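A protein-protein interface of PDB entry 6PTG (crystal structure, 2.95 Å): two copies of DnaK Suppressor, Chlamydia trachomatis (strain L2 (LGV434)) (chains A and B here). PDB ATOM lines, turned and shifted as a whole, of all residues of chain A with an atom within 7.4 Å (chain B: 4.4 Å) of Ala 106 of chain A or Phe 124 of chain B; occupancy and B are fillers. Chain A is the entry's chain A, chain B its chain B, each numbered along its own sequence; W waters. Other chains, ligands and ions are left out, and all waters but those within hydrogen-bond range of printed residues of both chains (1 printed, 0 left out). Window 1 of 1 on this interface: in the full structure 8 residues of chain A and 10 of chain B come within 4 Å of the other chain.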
ATOM      1  N   ARG A  22       4.801   4.550   1.931  1.00  0.00           N
ATOM      2  CA  ARG A  22       5.695   5.686   2.112  1.00  0.00           C
ATOM      3  C   ARG A  22       7.135   5.305   1.797  1.00  0.00           C
ATOM      4  O   ARG A  22       7.850   6.056   1.125  1.00  0.00           O
ATOM      5  CB  ARG A  22       5.577   6.231   3.535  1.00  0.00           C
ATOM      6  CG  ARG A  22       4.204   6.773   3.873  1.00  0.00           C
ATOM      7  CD  ARG A  22       4.179   7.338   5.269  1.00  0.00           C
ATOM      8  NE  ARG A  22       5.149   8.414   5.391  1.00  0.00           N
ATOM      9  CZ  ARG A  22       5.502   8.977   6.539  1.00  0.00           C
ATOM     10  NH1 ARG A  22       6.397   9.952   6.544  1.00  0.00           N
ATOM     11  NH2 ARG A  22       4.961   8.563   7.677  1.00  0.00           N
ATOM     12  N   ILE A 103       9.849   0.932  18.786  1.00  0.00           N
ATOM     13  CA  ILE A 103      10.208   2.260  18.276  1.00  0.00           C
ATOM     14  C   ILE A 103       8.996   3.174  18.416  1.00  0.00           C
ATOM     15  O   ILE A 103       7.906   2.825  17.926  1.00  0.00           O
ATOM     16  CB  ILE A 103      10.659   2.160  16.814  1.00  0.00           C
ATOM     17  CG1 ILE A 103      11.696   1.043  16.652  1.00  0.00           C
ATOM     18  CG2 ILE A 103      11.224   3.495  16.340  1.00  0.00           C
ATOM     19  CD1 ILE A 103      12.183   0.847  15.240  1.00  0.00           C
ATOM     20  N   PRO A 104       9.123   4.337  19.059  1.00  0.00           N
ATOM     21  CA  PRO A 104       7.941   5.178  19.300  1.00  0.00           C
ATOM     22  C   PRO A 104       7.247   5.575  18.007  1.00  0.00           C
ATOM     23  O   PRO A 104       7.891   5.889  17.003  1.00  0.00           O
ATOM     24  CB  PRO A 104       8.522   6.395  20.026  1.00  0.00           C
ATOM     25  CG  PRO A 104       9.736   5.856  20.711  1.00  0.00           C
ATOM     26  CD  PRO A 104      10.316   4.856  19.753  1.00  0.00           C
ATOM     27  N   LEU A 105       5.911   5.556  18.047  1.00  0.00           N
ATOM     28  CA  LEU A 105       5.117   5.811  16.848  1.00  0.00           C
ATOM     29  C   LEU A 105       5.408   7.195  16.277  1.00  0.00           C
ATOM     30  O   LEU A 105       5.406   7.385  15.054  1.00  0.00           O
ATOM     31  CB  LEU A 105       3.628   5.638  17.162  1.00  0.00           C
ATOM     32  CG  LEU A 105       2.588   5.912  16.067  1.00  0.00           C
ATOM     33  CD1 LEU A 105       2.926   5.199  14.763  1.00  0.00           C
ATOM     34  CD2 LEU A 105       1.200   5.511  16.548  1.00  0.00           C
ATOM     35  N   ALA A 106       5.672   8.176  17.144  1.00  0.00           N
ATOM     36  CA  ALA A 106       6.031   9.506  16.661  1.00  0.00           C
ATOM     37  C   ALA A 106       7.287   9.461  15.798  1.00  0.00           C
ATOM     38  O   ALA A 106       7.378  10.160  14.780  1.00  0.00           O
ATOM     39  CB  ALA A 106       6.234  10.452  17.841  1.00  0.00           C
ATOM     40  N   ARG A 107       8.276   8.662  16.204  1.00  0.00           N
ATOM     41  CA  ARG A 107       9.506   8.527  15.432  1.00  0.00           C
ATOM     42  C   ARG A 107       9.249   7.856  14.085  1.00  0.00           C
ATOM     43  O   ARG A 107       9.794   8.281  13.060  1.00  0.00           O
ATOM     44  CB  ARG A 107      10.534   7.738  16.246  1.00  0.00           C
ATOM     45  CG  ARG A 107      11.868   7.560  15.566  1.00  0.00           C
ATOM     46  CD  ARG A 107      12.903   7.110  16.563  1.00  0.00           C
ATOM     47  NE  ARG A 107      14.045   6.475  15.915  1.00  0.00           N
ATOM     48  CZ  ARG A 107      15.116   7.129  15.482  1.00  0.00           C
ATOM     49  NH1 ARG A 107      15.193   8.443  15.624  1.00  0.00           N
ATOM     50  NH2 ARG A 107      16.111   6.470  14.911  1.00  0.00           N
ATOM     51  N   LEU A 108       8.430   6.799  14.069  1.00  0.00           N
ATOM     52  CA  LEU A 108       8.106   6.134  12.811  1.00  0.00           C
ATOM     53  C   LEU A 108       7.273   7.033  11.911  1.00  0.00           C
ATOM     54  O   LEU A 108       7.444   7.024  10.688  1.00  0.00           O
ATOM     55  CB  LEU A 108       7.377   4.814  13.073  1.00  0.00           C
ATOM     56  CG  LEU A 108       8.165   3.738  13.812  1.00  0.00           C
ATOM     57  CD1 LEU A 108       7.253   2.612  14.271  1.00  0.00           C
ATOM     58  CD2 LEU A 108       9.264   3.209  12.912  1.00  0.00           C
ATOM     59  N   MET A 109       6.355   7.801  12.499  1.00  0.00           N
ATOM     60  CA  MET A 109       5.507   8.681  11.706  1.00  0.00           C
ATOM     61  C   MET A 109       6.343   9.739  10.994  1.00  0.00           C
ATOM     62  O   MET A 109       6.125  10.026   9.812  1.00  0.00           O
ATOM     63  CB  MET A 109       4.465   9.338  12.609  1.00  0.00           C
ATOM     64  CG  MET A 109       3.411  10.134  11.874  1.00  0.00           C
ATOM     65  SD  MET A 109       2.415   9.046  10.841  1.00  0.00           S
ATOM     66  CE  MET A 109       1.909   7.833  12.052  1.00  0.00           C
ATOM     67  N   ALA A 110       7.327  10.306  11.692  1.00  0.00           N
ATOM     68  CA  ALA A 110       8.200  11.299  11.081  1.00  0.00           C
ATOM     69  C   ALA A 110       9.273  10.655  10.210  1.00  0.00           C
ATOM     70  O   ALA A 110       9.548  11.137   9.105  1.00  0.00           O
ATOM     71  CB  ALA A 110       8.846  12.163  12.168  1.00  0.00           C
ATOM     72  N   ILE A 111       9.869   9.563  10.679  1.00  0.00           N
ATOM     73  CA  ILE A 111      10.963   8.895   9.977  1.00  0.00           C
ATOM     74  C   ILE A 111      10.544   7.459   9.691  1.00  0.00           C
ATOM     75  O   ILE A 111      10.897   6.548  10.451  1.00  0.00           O
ATOM     76  CB  ILE A 111      12.259   8.948  10.803  1.00  0.00           C
ATOM     77  CG1 ILE A 111      12.501  10.363  11.323  1.00  0.00           C
ATOM     78  CG2 ILE A 111      13.449   8.483   9.991  1.00  0.00           C
ATOM     79  CD1 ILE A 111      13.830  10.532  12.031  1.00  0.00           C
ATOM     80  N   PRO A 112       9.816   7.202   8.601  1.00  0.00           N
ATOM     81  CA  PRO A 112       9.282   5.848   8.378  1.00  0.00           C
ATOM     82  C   PRO A 112      10.346   4.788   8.124  1.00  0.00           C
ATOM     83  O   PRO A 112      10.027   3.599   8.215  1.00  0.00           O
ATOM     84  CB  PRO A 112       8.363   6.032   7.165  1.00  0.00           C
ATOM     85  CG  PRO A 112       8.921   7.222   6.460  1.00  0.00           C
ATOM     86  CD  PRO A 112       9.407   8.134   7.539  1.00  0.00           C
ATOM     87  N   VAL B  98      11.386  12.477  18.089  1.00  0.00           N
ATOM     88  CA  VAL B  98      11.693  11.918  16.775  1.00  0.00           C
ATOM     89  C   VAL B  98      13.183  11.665  16.613  1.00  0.00           C
ATOM     90  O   VAL B  98      13.602  10.569  16.235  1.00  0.00           O
ATOM     91  CB  VAL B  98      11.161  12.845  15.661  1.00  0.00           C
ATOM     92  CG1 VAL B  98      11.668  12.380  14.316  1.00  0.00           C
ATOM     93  CG2 VAL B  98       9.652  12.883  15.677  1.00  0.00           C
ATOM     94  N   MET B 116       9.033  17.903  20.177  1.00  0.00           N
ATOM     95  CA  MET B 116       9.892  17.630  19.040  1.00  0.00           C
ATOM     96  C   MET B 116      10.605  18.917  18.656  1.00  0.00           C
ATOM     97  O   MET B 116      10.138  20.018  18.953  1.00  0.00           O
ATOM     98  CB  MET B 116       9.086  17.098  17.846  1.00  0.00           C
ATOM     99  CG  MET B 116       8.303  15.841  18.131  1.00  0.00           C
ATOM    100  SD  MET B 116       7.131  15.476  16.828  1.00  0.00           S
ATOM    101  CE  MET B 116       5.730  16.452  17.384  1.00  0.00           C
ATOM    102  N   SER B 120      11.627  18.214  13.267  1.00  0.00           N
ATOM    103  CA  SER B 120      11.008  16.906  13.481  1.00  0.00           C
ATOM    104  C   SER B 120       9.493  17.007  13.505  1.00  0.00           C
ATOM    105  O   SER B 120       8.802  16.097  13.040  1.00  0.00           O
ATOM    106  CB  SER B 120      11.507  16.269  14.776  1.00  0.00           C
ATOM    107  OG  SER B 120      12.876  15.899  14.689  1.00  0.00           O
ATOM    108  N   GLN B 121       8.953  18.107  14.037  1.00  0.00           N
ATOM    109  CA  GLN B 121       7.506  18.277  14.009  1.00  0.00           C
ATOM    110  C   GLN B 121       7.004  18.422  12.580  1.00  0.00           C
ATOM    111  O   GLN B 121       5.942  17.894  12.235  1.00  0.00           O
ATOM    112  CB  GLN B 121       7.092  19.494  14.831  1.00  0.00           C
ATOM    113  CG  GLN B 121       5.626  19.470  15.229  1.00  0.00           C
ATOM    114  CD  GLN B 121       5.184  20.723  15.951  1.00  0.00           C
ATOM    115  OE1 GLN B 121       5.995  21.443  16.530  1.00  0.00           O
ATOM    116  NE2 GLN B 121       3.882  20.985  15.933  1.00  0.00           N
ATOM    117  N   GLU B 122       7.775  19.102  11.729  1.00  0.00           N
ATOM    118  CA  GLU B 122       7.442  19.190  10.311  1.00  0.00           C
ATOM    119  C   GLU B 122       7.361  17.803   9.682  1.00  0.00           C
ATOM    120  O   GLU B 122       6.378  17.471   9.010  1.00  0.00           O
ATOM    121  CB  GLU B 122       8.477  20.061   9.602  1.00  0.00           C
ATOM    122  CG  GLU B 122       8.062  21.518   9.512  1.00  0.00           C
ATOM    123  CD  GLU B 122       9.134  22.395   8.901  1.00  0.00           C
ATOM    124  OE1 GLU B 122       9.637  22.055   7.809  1.00  0.00           O
ATOM    125  OE2 GLU B 122       9.464  23.433   9.515  1.00  0.00           O
ATOM    126  N   LYS B 123       8.403  16.983   9.876  1.00  0.00           N
ATOM    127  CA  LYS B 123       8.376  15.614   9.371  1.00  0.00           C
ATOM    128  C   LYS B 123       7.196  14.833   9.945  1.00  0.00           C
ATOM    129  O   LYS B 123       6.524  14.086   9.222  1.00  0.00           O
ATOM    130  CB  LYS B 123       9.683  14.891   9.704  1.00  0.00           C
ATOM    131  CG  LYS B 123      10.926  15.325   8.940  1.00  0.00           C
ATOM    132  CD  LYS B 123      12.137  14.521   9.431  1.00  0.00           C
ATOM    133  CE  LYS B 123      13.470  15.153   9.051  1.00  0.00           C
ATOM    134  NZ  LYS B 123      13.679  15.233   7.582  1.00  0.00           N
ATOM    135  N   PHE B 124       6.930  14.991  11.243  1.00  0.00           N
ATOM    136  CA  PHE B 124       5.830  14.268  11.879  1.00  0.00           C
ATOM    137  C   PHE B 124       4.475  14.681  11.306  1.00  0.00           C
ATOM    138  O   PHE B 124       3.658  13.824  10.947  1.00  0.00           O
ATOM    139  CB  PHE B 124       5.878  14.489  13.390  1.00  0.00           C
ATOM    140  CG  PHE B 124       4.705  13.916  14.126  1.00  0.00           C
ATOM    141  CD1 PHE B 124       4.661  12.570  14.443  1.00  0.00           C
ATOM    142  CD2 PHE B 124       3.648  14.727  14.511  1.00  0.00           C
ATOM    143  CE1 PHE B 124       3.581  12.036  15.126  1.00  0.00           C
ATOM    144  CE2 PHE B 124       2.570  14.205  15.194  1.00  0.00           C
ATOM    145  CZ  PHE B 124       2.536  12.854  15.503  1.00  0.00           C
ATOM    146  N   GLU B 125       4.216  15.992  11.215  1.00  0.00           N
ATOM    147  CA  GLU B 125       2.922  16.459  10.715  1.00  0.00           C
ATOM    148  C   GLU B 125       2.688  16.002   9.279  1.00  0.00           C
ATOM    149  O   GLU B 125       1.560  15.661   8.904  1.00  0.00           O
ATOM    150  CB  GLU B 125       2.837  17.988  10.785  1.00  0.00           C
ATOM    151  CG  GLU B 125       2.984  18.633  12.165  1.00  0.00           C
ATOM    152  CD  GLU B 125       1.774  18.468  13.058  1.00  0.00           C
ATOM    153  OE1 GLU B 125       0.731  17.971  12.581  1.00  0.00           O
ATOM    154  OE2 GLU B 125       1.868  18.859  14.244  1.00  0.00           O
ATOM    155  N   LYS B 126       3.740  16.004   8.458  1.00  0.00           N
ATOM    156  CA  LYS B 126       3.611  15.535   7.082  1.00  0.00           C
ATOM    157  C   LYS B 126       3.308  14.043   7.024  1.00  0.00           C
ATOM    158  O   LYS B 126       2.591  13.594   6.120  1.00  0.00           O
ATOM    159  CB  LYS B 126       4.878  15.870   6.293  1.00  0.00           C
ATOM    160  CG  LYS B 126       4.835  15.428   4.842  1.00  0.00           C
ATOM    161  CD  LYS B 126       5.925  16.099   4.026  1.00  0.00           C
ATOM    162  CE  LYS B 126       6.151  15.391   2.695  1.00  0.00           C
ATOM    163  NZ  LYS B 126       7.283  15.997   1.938  1.00  0.00           N
ATOM    164  N   GLY B 127       3.841  13.262   7.969  1.00  0.00           N
ATOM    165  CA  GLY B 127       3.562  11.836   7.987  1.00  0.00           C
ATOM    166  C   GLY B 127       2.105  11.509   8.262  1.00  0.00           C
ATOM    167  O   GLY B 127       1.546  10.580   7.670  1.00  0.00           O
ATOM    168  N   LEU B 128       1.466  12.271   9.156  1.00  0.00           N
ATOM    169  CA  LEU B 128       0.054  12.054   9.466  1.00  0.00           C
ATOM    170  C   LEU B 128      -0.859  12.215   8.255  1.00  0.00           C
ATOM    171  O   LEU B 128      -1.966  11.665   8.254  1.00  0.00           O
ATOM    172  CB  LEU B 128      -0.404  13.015  10.558  1.00  0.00           C
ATOM    173  CG  LEU B 128       0.186  12.827  11.949  1.00  0.00           C
ATOM    174  CD1 LEU B 128      -0.340  13.901  12.869  1.00  0.00           C
ATOM    175  CD2 LEU B 128      -0.137  11.454  12.488  1.00  0.00           C
HETATM  176  O   HOH W   1       7.551  12.492   7.106  1.00  0.00           O
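NH2 of Arg 22 of chain A touches CA of Gly 127 of chain B (3.6 Å). Ala 106 of chain A touches Val 98 of chain B (O to CG2, 3.7 Å). Ala 106 of chain A touches Phe 124 of chain B. CD1 of Phe 124 of chain B touches CB of Met 109 of chain A, at 3.7 Å. CB of Ala 110 of chain A touches CG1 of Val 98 of chain B, 3.6 Å away. Ala 110 of chain A touches Lys 123 of chain B. N of Phe 124 of chain B touches CB of Ala 110 of chain A (3.5 Å). Ile 111 of chain A touches Val 98 of chain B (CD1 to CG1, 3.6 Å).
Printed residues of chain B that touch a printed residue of chain A: Val 98, Lys 123, Phe 124, Gly 127 and Leu 128. Hydrophobic or aromatic side chains of chain B that line the printed part of chain A: Val 98, Phe 124 and Leu 128. Among the printed residues, no Asp or Glu carboxylate lies within 4 Å of a Lys or Arg side-chain nitrogen of the other chain.
Of chain B, only Val 98 and Phe 124 come within 4 Å of Ala 106 of chain A. Phe 124 of chain B touches three residues of chain A. Lys 126 of chain B touches none of the printed residues of chain A. Of the printed residues of chain A, Gly 127 of chain B touches Arg 22 and Met 109. Printed residues of chain A within 4 Å of Leu 128 of chain B: Met 109. The nearest residue of chain A that does not touch Phe 124 of chain B is Leu 105 of chain A (5.0 Å).
Water W1 lies within hydrogen-bond range of the backbone carbonyl oxygen (O) of Lys 123 of chain B, the guanidinium group (NH1) of Arg 22 of chain A and the backbone carbonyl oxygen (O) of Ala 110 of chain A.
No position is printed for both chains.
N of Leu 128 of chain B lies within hydrogen-bond range of SD of Met 109 of chain A (3.8 Å). The side-chain sulfur (SD) of Met 109 of chain A lies close to the backbone carbonyl oxygen (O) of Gly 127 of chain B (3.6 Å). The backbone carbonyl oxygen (O) of Val 98 of chain B sits at hydrogen-bond distance from the guanidinium group (NH1) of Arg 107 of chain A (2.7 Å).
NH2 of Arg 22 of chain A sits at hydrogen-bond distance from O of Met 109 of chain A.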
